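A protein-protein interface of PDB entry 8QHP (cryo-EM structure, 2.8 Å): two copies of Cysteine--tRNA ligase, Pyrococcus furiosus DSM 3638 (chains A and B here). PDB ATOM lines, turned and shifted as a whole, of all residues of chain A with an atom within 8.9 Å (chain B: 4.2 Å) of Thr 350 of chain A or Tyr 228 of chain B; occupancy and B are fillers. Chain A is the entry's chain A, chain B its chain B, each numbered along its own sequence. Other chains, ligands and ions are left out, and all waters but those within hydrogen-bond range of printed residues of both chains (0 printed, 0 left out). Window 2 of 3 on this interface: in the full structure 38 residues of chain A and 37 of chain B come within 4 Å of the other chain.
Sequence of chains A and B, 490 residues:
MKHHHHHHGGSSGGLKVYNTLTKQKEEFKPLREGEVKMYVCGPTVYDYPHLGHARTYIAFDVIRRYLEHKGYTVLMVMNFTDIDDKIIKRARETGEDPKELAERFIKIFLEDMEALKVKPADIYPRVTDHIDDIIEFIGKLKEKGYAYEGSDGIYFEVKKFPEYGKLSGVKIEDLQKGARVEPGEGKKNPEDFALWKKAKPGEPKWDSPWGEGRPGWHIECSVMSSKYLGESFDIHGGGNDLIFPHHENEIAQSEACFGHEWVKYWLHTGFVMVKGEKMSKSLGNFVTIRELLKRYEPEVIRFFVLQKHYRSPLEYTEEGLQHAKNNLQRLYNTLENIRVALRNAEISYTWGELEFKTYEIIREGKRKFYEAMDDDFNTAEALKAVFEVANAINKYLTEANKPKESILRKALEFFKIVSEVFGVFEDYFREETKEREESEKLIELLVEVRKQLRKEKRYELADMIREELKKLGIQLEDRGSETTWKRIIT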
ATOM      1  N   GLU A 346      30.133  11.047  15.175  1.00  0.00           N
ATOM      2  CA  GLU A 346      30.367  11.656  16.473  1.00  0.00           C
ATOM      3  C   GLU A 346      29.112  11.559  17.328  1.00  0.00           C
ATOM      4  O   GLU A 346      28.009  11.324  16.828  1.00  0.00           O
ATOM      5  CB  GLU A 346      30.792  13.118  16.320  1.00  0.00           C
ATOM      6  CG  GLU A 346      29.756  13.991  15.640  1.00  0.00           C
ATOM      7  CD  GLU A 346      30.383  15.136  14.876  1.00  0.00           C
ATOM      8  OE1 GLU A 346      31.487  14.945  14.324  1.00  0.00           O
ATOM      9  OE2 GLU A 346      29.776  16.227  14.828  1.00  0.00           O
ATOM     10  N   ILE A 347      29.294  11.737  18.636  1.00  0.00           N
ATOM     11  CA  ILE A 347      28.157  11.704  19.543  1.00  0.00           C
ATOM     12  C   ILE A 347      27.289  12.933  19.306  1.00  0.00           C
ATOM     13  O   ILE A 347      27.758  13.975  18.830  1.00  0.00           O
ATOM     14  CB  ILE A 347      28.617  11.621  21.009  1.00  0.00           C
ATOM     15  CG1 ILE A 347      29.168  12.965  21.476  1.00  0.00           C
ATOM     16  CG2 ILE A 347      29.666  10.536  21.176  1.00  0.00           C
ATOM     17  CD1 ILE A 347      29.444  13.011  22.952  1.00  0.00           C
ATOM     18  N   SER A 348      26.008  12.809  19.629  1.00  0.00           N
ATOM     19  CA  SER A 348      25.028  13.846  19.339  1.00  0.00           C
ATOM     20  C   SER A 348      24.705  14.606  20.618  1.00  0.00           C
ATOM     21  O   SER A 348      24.028  14.079  21.508  1.00  0.00           O
ATOM     22  CB  SER A 348      23.768  13.239  18.728  1.00  0.00           C
ATOM     23  OG  SER A 348      23.285  12.169  19.518  1.00  0.00           O
ATOM     24  N   TYR A 349      25.187  15.845  20.709  1.00  0.00           N
ATOM     25  CA  TYR A 349      24.764  16.734  21.780  1.00  0.00           C
ATOM     26  C   TYR A 349      23.411  17.363  21.495  1.00  0.00           C
ATOM     27  O   TYR A 349      22.793  17.923  22.408  1.00  0.00           O
ATOM     28  CB  TYR A 349      25.800  17.835  22.004  1.00  0.00           C
ATOM     29  CG  TYR A 349      27.153  17.327  22.440  1.00  0.00           C
ATOM     30  CD1 TYR A 349      27.350  16.842  23.723  1.00  0.00           C
ATOM     31  CD2 TYR A 349      28.233  17.345  21.572  1.00  0.00           C
ATOM     32  CE1 TYR A 349      28.584  16.379  24.126  1.00  0.00           C
ATOM     33  CE2 TYR A 349      29.472  16.885  21.967  1.00  0.00           C
ATOM     34  CZ  TYR A 349      29.642  16.405  23.246  1.00  0.00           C
ATOM     35  OH  TYR A 349      30.875  15.945  23.643  1.00  0.00           O
ATOM     36  N   THR A 350      22.945  17.287  20.252  1.00  0.00           N
ATOM     37  CA  THR A 350      21.630  17.778  19.873  1.00  0.00           C
ATOM     38  C   THR A 350      21.201  17.059  18.604  1.00  0.00           C
ATOM     39  O   THR A 350      22.026  16.492  17.883  1.00  0.00           O
ATOM     40  CB  THR A 350      21.629  19.295  19.658  1.00  0.00           C
ATOM     41  OG1 THR A 350      20.306  19.729  19.318  1.00  0.00           O
ATOM     42  CG2 THR A 350      22.582  19.674  18.538  1.00  0.00           C
ATOM     43  N   TRP A 351      19.900  17.085  18.344  1.00  0.00           N
ATOM     44  CA  TRP A 351      19.327  16.480  17.152  1.00  0.00           C
ATOM     45  C   TRP A 351      18.553  17.530  16.373  1.00  0.00           C
ATOM     46  O   TRP A 351      17.703  18.227  16.938  1.00  0.00           O
ATOM     47  CB  TRP A 351      18.411  15.308  17.507  1.00  0.00           C
ATOM     48  CG  TRP A 351      19.106  13.985  17.567  1.00  0.00           C
ATOM     49  CD1 TRP A 351      20.450  13.762  17.542  1.00  0.00           C
ATOM     50  CD2 TRP A 351      18.487  12.697  17.652  1.00  0.00           C
ATOM     51  NE1 TRP A 351      20.706  12.415  17.612  1.00  0.00           N
ATOM     52  CE2 TRP A 351      19.516  11.739  17.679  1.00  0.00           C
ATOM     53  CE3 TRP A 351      17.160  12.262  17.710  1.00  0.00           C
ATOM     54  CZ2 TRP A 351      19.262  10.374  17.762  1.00  0.00           C
ATOM     55  CZ3 TRP A 351      16.910  10.907  17.791  1.00  0.00           C
ATOM     56  CH2 TRP A 351      17.956   9.979  17.816  1.00  0.00           C
ATOM     57  N   GLY A 352      18.847  17.639  15.081  1.00  0.00           N
ATOM     58  CA  GLY A 352      18.115  18.516  14.196  1.00  0.00           C
ATOM     59  C   GLY A 352      16.858  17.856  13.673  1.00  0.00           C
ATOM     60  O   GLY A 352      16.448  16.782  14.114  1.00  0.00           O
ATOM     61  N   GLU A 353      16.229  18.527  12.709  1.00  0.00           N
ATOM     62  CA  GLU A 353      15.031  17.966  12.096  1.00  0.00           C
ATOM     63  C   GLU A 353      15.352  16.725  11.276  1.00  0.00           C
ATOM     64  O   GLU A 353      14.540  15.794  11.218  1.00  0.00           O
ATOM     65  CB  GLU A 353      14.342  19.020  11.231  1.00  0.00           C
ATOM     66  CG  GLU A 353      12.976  18.598  10.725  1.00  0.00           C
ATOM     67  CD  GLU A 353      12.244  19.719  10.019  1.00  0.00           C
ATOM     68  OE1 GLU A 353      12.796  20.834   9.924  1.00  0.00           O
ATOM     69  OE2 GLU A 353      11.104  19.481   9.556  1.00  0.00           O
ATOM     70  N   GLU A 355      17.768  14.470  11.887  1.00  0.00           N
ATOM     71  CA  GLU A 355      17.978  13.340  12.786  1.00  0.00           C
ATOM     72  C   GLU A 355      16.655  12.800  13.309  1.00  0.00           C
ATOM     73  O   GLU A 355      16.462  11.582  13.385  1.00  0.00           O
ATOM     74  CB  GLU A 355      18.886  13.744  13.948  1.00  0.00           C
ATOM     75  CG  GLU A 355      20.358  13.825  13.593  1.00  0.00           C
ATOM     76  CD  GLU A 355      20.708  15.081  12.825  1.00  0.00           C
ATOM     77  OE1 GLU A 355      19.889  16.022  12.819  1.00  0.00           O
ATOM     78  OE2 GLU A 355      21.804  15.127  12.227  1.00  0.00           O
ATOM     79  N   PHE A 356      15.729  13.690  13.672  1.00  0.00           N
ATOM     80  CA  PHE A 356      14.428  13.233  14.146  1.00  0.00           C
ATOM     81  C   PHE A 356      13.637  12.557  13.035  1.00  0.00           C
ATOM     82  O   PHE A 356      12.952  11.559  13.277  1.00  0.00           O
ATOM     83  CB  PHE A 356      13.638  14.397  14.741  1.00  0.00           C
ATOM     84  CG  PHE A 356      13.911  14.624  16.197  1.00  0.00           C
ATOM     85  CD1 PHE A 356      13.364  13.786  17.154  1.00  0.00           C
ATOM     86  CD2 PHE A 356      14.716  15.669  16.611  1.00  0.00           C
ATOM     87  CE1 PHE A 356      13.615  13.989  18.495  1.00  0.00           C
ATOM     88  CE2 PHE A 356      14.969  15.878  17.951  1.00  0.00           C
ATOM     89  CZ  PHE A 356      14.418  15.035  18.894  1.00  0.00           C
ATOM     90  N   TYR A 359      15.164   9.097  12.667  1.00  0.00           N
ATOM     91  CA  TYR A 359      14.790   8.261  13.801  1.00  0.00           C
ATOM     92  C   TYR A 359      13.340   7.813  13.699  1.00  0.00           C
ATOM     93  O   TYR A 359      13.020   6.656  13.993  1.00  0.00           O
ATOM     94  CB  TYR A 359      15.022   9.009  15.113  1.00  0.00           C
ATOM     95  CG  TYR A 359      14.269   8.418  16.287  1.00  0.00           C
ATOM     96  CD1 TYR A 359      14.735   7.282  16.933  1.00  0.00           C
ATOM     97  CD2 TYR A 359      13.095   8.998  16.747  1.00  0.00           C
ATOM     98  CE1 TYR A 359      14.050   6.740  18.002  1.00  0.00           C
ATOM     99  CE2 TYR A 359      12.406   8.464  17.814  1.00  0.00           C
ATOM    100  CZ  TYR A 359      12.887   7.335  18.438  1.00  0.00           C
ATOM    101  OH  TYR A 359      12.201   6.802  19.503  1.00  0.00           O
ATOM    102  N   GLU A 360      12.446   8.717  13.295  1.00  0.00           N
ATOM    103  CA  GLU A 360      11.045   8.347  13.150  1.00  0.00           C
ATOM    104  C   GLU A 360      10.868   7.289  12.074  1.00  0.00           C
ATOM    105  O   GLU A 360      10.104   6.335  12.253  1.00  0.00           O
ATOM    106  CB  GLU A 360      10.201   9.582  12.839  1.00  0.00           C
ATOM    107  CG  GLU A 360       9.999  10.501  14.029  1.00  0.00           C
ATOM    108  CD  GLU A 360       9.230   9.839  15.153  1.00  0.00           C
ATOM    109  OE1 GLU A 360       8.370   8.979  14.865  1.00  0.00           O
ATOM    110  OE2 GLU A 360       9.489  10.171  16.329  1.00  0.00           O
ATOM    111  N   TYR A 396      19.696  10.022   4.690  1.00  0.00           N
ATOM    112  CA  TYR A 396      20.323  10.698   5.820  1.00  0.00           C
ATOM    113  C   TYR A 396      21.828  10.829   5.622  1.00  0.00           C
ATOM    114  O   TYR A 396      22.405  11.888   5.887  1.00  0.00           O
ATOM    115  CB  TYR A 396      20.018   9.949   7.115  1.00  0.00           C
ATOM    116  CG  TYR A 396      20.819  10.432   8.301  1.00  0.00           C
ATOM    117  CD1 TYR A 396      20.504  11.623   8.936  1.00  0.00           C
ATOM    118  CD2 TYR A 396      21.888   9.695   8.786  1.00  0.00           C
ATOM    119  CE1 TYR A 396      21.233  12.068  10.020  1.00  0.00           C
ATOM    120  CE2 TYR A 396      22.623  10.132   9.868  1.00  0.00           C
ATOM    121  CZ  TYR A 396      22.291  11.318  10.481  1.00  0.00           C
ATOM    122  OH  TYR A 396      23.019  11.758  11.560  1.00  0.00           O
ATOM    123  N   LYS A 402      27.447  15.899   9.098  1.00  0.00           N
ATOM    124  CA  LYS A 402      28.162  15.085  10.071  1.00  0.00           C
ATOM    125  C   LYS A 402      27.201  14.065  10.667  1.00  0.00           C
ATOM    126  O   LYS A 402      26.380  14.414  11.526  1.00  0.00           O
ATOM    127  CB  LYS A 402      28.769  15.956  11.172  1.00  0.00           C
ATOM    128  CG  LYS A 402      30.173  16.455  10.883  1.00  0.00           C
ATOM    129  CD  LYS A 402      31.142  15.296  10.742  1.00  0.00           C
ATOM    130  CE  LYS A 402      32.570  15.724  11.043  1.00  0.00           C
ATOM    131  NZ  LYS A 402      33.028  16.843  10.176  1.00  0.00           N
ATOM    132  N   PRO A 403      27.258  12.809  10.229  1.00  0.00           N
ATOM    133  CA  PRO A 403      26.304  11.811  10.728  1.00  0.00           C
ATOM    134  C   PRO A 403      26.457  11.579  12.222  1.00  0.00           C
ATOM    135  O   PRO A 403      27.569  11.540  12.755  1.00  0.00           O
ATOM    136  CB  PRO A 403      26.657  10.549   9.931  1.00  0.00           C
ATOM    137  CG  PRO A 403      27.404  11.043   8.735  1.00  0.00           C
ATOM    138  CD  PRO A 403      28.148  12.256   9.196  1.00  0.00           C
ATOM    139  N   LYS A 404      25.322  11.423  12.896  1.00  0.00           N
ATOM    140  CA  LYS A 404      25.318  11.133  14.321  1.00  0.00           C
ATOM    141  C   LYS A 404      25.459   9.635  14.554  1.00  0.00           C
ATOM    142  O   LYS A 404      24.900   8.820  13.814  1.00  0.00           O
ATOM    143  CB  LYS A 404      24.035  11.649  14.971  1.00  0.00           C
ATOM    144  CG  LYS A 404      23.814  13.142  14.810  1.00  0.00           C
ATOM    145  CD  LYS A 404      24.981  13.938  15.367  1.00  0.00           C
ATOM    146  CE  LYS A 404      24.751  15.430  15.210  1.00  0.00           C
ATOM    147  NZ  LYS A 404      25.895  16.218  15.739  1.00  0.00           N
ATOM    148  N   GLU A 405      26.211   9.277  15.597  1.00  0.00           N
ATOM    149  CA  GLU A 405      26.476   7.872  15.877  1.00  0.00           C
ATOM    150  C   GLU A 405      25.225   7.139  16.343  1.00  0.00           C
ATOM    151  O   GLU A 405      25.070   5.945  16.062  1.00  0.00           O
ATOM    152  CB  GLU A 405      27.588   7.758  16.919  1.00  0.00           C
ATOM    153  CG  GLU A 405      28.026   6.340  17.221  1.00  0.00           C
ATOM    154  CD  GLU A 405      27.347   5.770  18.446  1.00  0.00           C
ATOM    155  OE1 GLU A 405      26.477   6.456  19.022  1.00  0.00           O
ATOM    156  OE2 GLU A 405      27.690   4.635  18.837  1.00  0.00           O
ATOM    157  N   SER A 406      24.329   7.830  17.055  1.00  0.00           N
ATOM    158  CA  SER A 406      23.127   7.177  17.565  1.00  0.00           C
ATOM    159  C   SER A 406      22.204   6.722  16.439  1.00  0.00           C
ATOM    160  O   SER A 406      21.631   5.628  16.506  1.00  0.00           O
ATOM    161  CB  SER A 406      22.393   8.112  18.526  1.00  0.00           C
ATOM    162  OG  SER A 406      22.240   9.410  17.972  1.00  0.00           O
ATOM    163  N   ILE A 407      22.036   7.547  15.402  1.00  0.00           N
ATOM    164  CA  ILE A 407      21.162   7.177  14.290  1.00  0.00           C
ATOM    165  C   ILE A 407      21.698   5.937  13.582  1.00  0.00           C
ATOM    166  O   ILE A 407      20.954   4.990  13.291  1.00  0.00           O
ATOM    167  CB  ILE A 407      21.007   8.361  13.320  1.00  0.00           C
ATOM    168  CG1 ILE A 407      20.269   9.511  14.000  1.00  0.00           C
ATOM    169  CG2 ILE A 407      20.279   7.931  12.064  1.00  0.00           C
ATOM    170  CD1 ILE A 407      18.854   9.175  14.386  1.00  0.00           C
ATOM    171  N   LEU B  75      14.454   5.580  22.791  1.00  0.00           N
ATOM    172  CA  LEU B  75      15.149   6.854  22.630  1.00  0.00           C
ATOM    173  C   LEU B  75      15.537   7.325  24.026  1.00  0.00           C
ATOM    174  O   LEU B  75      14.687   7.778  24.795  1.00  0.00           O
ATOM    175  CB  LEU B  75      14.269   7.871  21.913  1.00  0.00           C
ATOM    176  CG  LEU B  75      14.850   9.272  21.727  1.00  0.00           C
ATOM    177  CD1 LEU B  75      16.117   9.212  20.900  1.00  0.00           C
ATOM    178  CD2 LEU B  75      13.829  10.187  21.078  1.00  0.00           C
ATOM    179  N   ILE B 123      21.045  11.167  22.778  1.00  0.00           N
ATOM    180  CA  ILE B 123      21.279  12.604  22.825  1.00  0.00           C
ATOM    181  C   ILE B 123      21.933  12.947  24.154  1.00  0.00           C
ATOM    182  O   ILE B 123      21.562  12.401  25.198  1.00  0.00           O
ATOM    183  CB  ILE B 123      19.973  13.403  22.638  1.00  0.00           C
ATOM    184  CG1 ILE B 123      19.172  12.857  21.459  1.00  0.00           C
ATOM    185  CG2 ILE B 123      20.277  14.872  22.417  1.00  0.00           C
ATOM    186  CD1 ILE B 123      17.854  13.554  21.250  1.00  0.00           C
ATOM    187  N   PRO B 125      22.340  16.398  25.713  1.00  0.00           N
ATOM    188  CA  PRO B 125      22.189  17.854  25.756  1.00  0.00           C
ATOM    189  C   PRO B 125      23.031  18.474  26.858  1.00  0.00           C
ATOM    190  O   PRO B 125      23.279  17.869  27.903  1.00  0.00           O
ATOM    191  CB  PRO B 125      20.693  18.047  26.022  1.00  0.00           C
ATOM    192  CG  PRO B 125      20.275  16.798  26.707  1.00  0.00           C
ATOM    193  CD  PRO B 125      21.105  15.702  26.112  1.00  0.00           C
ATOM    194  N   HIS B 130      21.749  25.233  25.808  1.00  0.00           N
ATOM    195  CA  HIS B 130      20.297  25.367  25.881  1.00  0.00           C
ATOM    196  C   HIS B 130      19.908  26.504  26.812  1.00  0.00           C
ATOM    197  O   HIS B 130      18.908  26.424  27.532  1.00  0.00           O
ATOM    198  CB  HIS B 130      19.643  24.063  26.334  1.00  0.00           C
ATOM    199  CG  HIS B 130      19.826  22.930  25.374  1.00  0.00           C
ATOM    200  ND1 HIS B 130      21.030  22.281  25.209  1.00  0.00           N
ATOM    201  CD2 HIS B 130      18.957  22.333  24.524  1.00  0.00           C
ATOM    202  CE1 HIS B 130      20.895  21.332  24.300  1.00  0.00           C
ATOM    203  NE2 HIS B 130      19.648  21.344  23.868  1.00  0.00           N
ATOM    204  N   MET B 224      15.386  20.199  28.799  1.00  0.00           N
ATOM    205  CA  MET B 224      15.956  19.294  27.806  1.00  0.00           C
ATOM    206  C   MET B 224      15.023  18.128  27.510  1.00  0.00           C
ATOM    207  O   MET B 224      14.888  17.714  26.352  1.00  0.00           O
ATOM    208  CB  MET B 224      17.316  18.795  28.282  1.00  0.00           C
ATOM    209  CG  MET B 224      18.308  19.912  28.505  1.00  0.00           C
ATOM    210  SD  MET B 224      19.815  19.350  29.302  1.00  0.00           S
ATOM    211  CE  MET B 224      20.617  20.916  29.595  1.00  0.00           C
ATOM    212  N   SER B 225      14.378  17.578  28.542  1.00  0.00           N
ATOM    213  CA  SER B 225      13.447  16.476  28.333  1.00  0.00           C
ATOM    214  C   SER B 225      12.270  16.907  27.469  1.00  0.00           C
ATOM    215  O   SER B 225      11.894  16.210  26.523  1.00  0.00           O
ATOM    216  CB  SER B 225      12.965  15.944  29.681  1.00  0.00           C
ATOM    217  OG  SER B 225      12.344  16.971  30.434  1.00  0.00           O
ATOM    218  N   SER B 226      11.668  18.058  27.781  1.00  0.00           N
ATOM    219  CA  SER B 226      10.565  18.550  26.965  1.00  0.00           C
ATOM    220  C   SER B 226      11.016  18.875  25.549  1.00  0.00           C
ATOM    221  O   SER B 226      10.226  18.756  24.605  1.00  0.00           O
ATOM    222  CB  SER B 226       9.944  19.783  27.617  1.00  0.00           C
ATOM    223  OG  SER B 226       9.636  19.534  28.977  1.00  0.00           O
ATOM    224  N   LYS B 227      12.271  19.291  25.377  1.00  0.00           N
ATOM    225  CA  LYS B 227      12.746  19.649  24.046  1.00  0.00           C
ATOM    226  C   LYS B 227      12.965  18.415  23.179  1.00  0.00           C
ATOM    227  O   LYS B 227      12.587  18.396  22.001  1.00  0.00           O
ATOM    228  CB  LYS B 227      14.035  20.459  24.148  1.00  0.00           C
ATOM    229  CG  LYS B 227      14.594  20.851  22.791  1.00  0.00           C
ATOM    230  CD  LYS B 227      15.944  21.513  22.926  1.00  0.00           C
ATOM    231  CE  LYS B 227      16.496  21.890  21.563  1.00  0.00           C
ATOM    232  NZ  LYS B 227      15.683  22.953  20.922  1.00  0.00           N
ATOM    233  N   TYR B 228      13.590  17.377  23.734  1.00  0.00           N
ATOM    234  CA  TYR B 228      14.041  16.262  22.910  1.00  0.00           C
ATOM    235  C   TYR B 228      13.156  15.025  22.979  1.00  0.00           C
ATOM    236  O   TYR B 228      13.235  14.182  22.079  1.00  0.00           O
ATOM    237  CB  TYR B 228      15.472  15.867  23.289  1.00  0.00           C
ATOM    238  CG  TYR B 228      16.490  16.915  22.924  1.00  0.00           C
ATOM    239  CD1 TYR B 228      16.822  17.150  21.599  1.00  0.00           C
ATOM    240  CD2 TYR B 228      17.118  17.669  23.902  1.00  0.00           C
ATOM    241  CE1 TYR B 228      17.751  18.109  21.257  1.00  0.00           C
ATOM    242  CE2 TYR B 228      18.051  18.627  23.570  1.00  0.00           C
ATOM    243  CZ  TYR B 228      18.364  18.845  22.246  1.00  0.00           C
ATOM    244  OH  TYR B 228      19.292  19.801  21.910  1.00  0.00           O
ATOM    245  N   LEU B 229      12.317  14.888  24.005  1.00  0.00           N
ATOM    246  CA  LEU B 229      11.480  13.708  24.166  1.00  0.00           C
ATOM    247  C   LEU B 229       9.997  14.020  24.006  1.00  0.00           C
ATOM    248  O   LEU B 229       9.151  13.216  24.408  1.00  0.00           O
ATOM    249  CB  LEU B 229      11.740  13.056  25.524  1.00  0.00           C
ATOM    250  CG  LEU B 229      13.086  12.348  25.678  1.00  0.00           C
ATOM    251  CD1 LEU B 229      13.193  11.721  27.051  1.00  0.00           C
ATOM    252  CD2 LEU B 229      13.256  11.301  24.595  1.00  0.00           C
ATOM    253  N   GLY B 230       9.664  15.166  23.433  1.00  0.00           N
ATOM    254  CA  GLY B 230       8.277  15.525  23.248  1.00  0.00           C
ATOM    255  C   GLY B 230       7.663  16.134  24.489  1.00  0.00           C
ATOM    256  O   GLY B 230       8.324  16.423  25.491  1.00  0.00           O
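The side-chain hydroxyl (OG1) of Thr 350 of chain A lies within hydrogen-bond range of the side-chain hydroxyl (OH) of Tyr 228 of chain B.
The side-chain hydroxyl (OG) of Ser 348 of chain A lies within hydrogen-bond range of the indole nitrogen (NE1) of Trp 351 of chain A.
The side-chain hydroxyl (OG) of Ser 348 of chain A is in hydrogen-bond range of the side-chain hydroxyl (OG) of Ser 406 of chain A (3.3 Å).
OG of Ser 406 of chain A sits close to NE1 of Trp 351 of chain A, at 3.4 Å.
NE2 of His 130 of chain B sits at hydrogen-bond distance from OH of Tyr 228 of chain B.
Ser 348 of chain A touches Ile 123 of chain B (O to CA, 3.4 Å).
Ile 123 of chain B touches Tyr 349 of chain A (CG2 to O, 3.95 Å).
O of Tyr 349 of chain A touches CA of Pro 125 of chain B, at 3.4 Å.
Trp 351 of chain A touches Leu 75 of chain B (CZ3 to CD1, 3.6 Å).
CD1 of Ile 123 of chain B touches CD2 of Trp 351 of chain A (3.8 Å).
CE1 of Tyr 228 of chain B touches N of Trp 351 of chain A, at 3.8 Å.
CZ of Phe 356 of chain A touches O of Tyr 228 of chain B, at 3.5 Å.
OH of Tyr 359 of chain A touches CB of Leu 75 of chain B (3.4 Å).
Of the printed residues of chain B, Tyr 349 of chain A touches Ile 123 and Pro 125.
Printed residues of chain B within 4 Å of Thr 350 of chain A: Tyr 228 (2.8 Å).
Printed residues of chain B within 4 Å of Tyr 359 of chain A: Leu 75 (3.4 Å).
Of the printed residues of chain A, Leu 75 of chain B touches Trp 351 (3.6 Å) and Tyr 359 (3.4 Å).
Printed residues of chain A within 4 Å of Tyr 228 of chain B: Thr 350, Trp 351 and Phe 356.
Printed residues of chain A that touch a printed residue of chain B: Ser 348, Tyr 349, Thr 350, Trp 351, Phe 356 and Tyr 359.
Hydrophobic or aromatic side chains of chain A within 4 Å of the printed part of chain B: Trp 351, Phe 356 and Tyr 359.
No position is printed for both chains.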
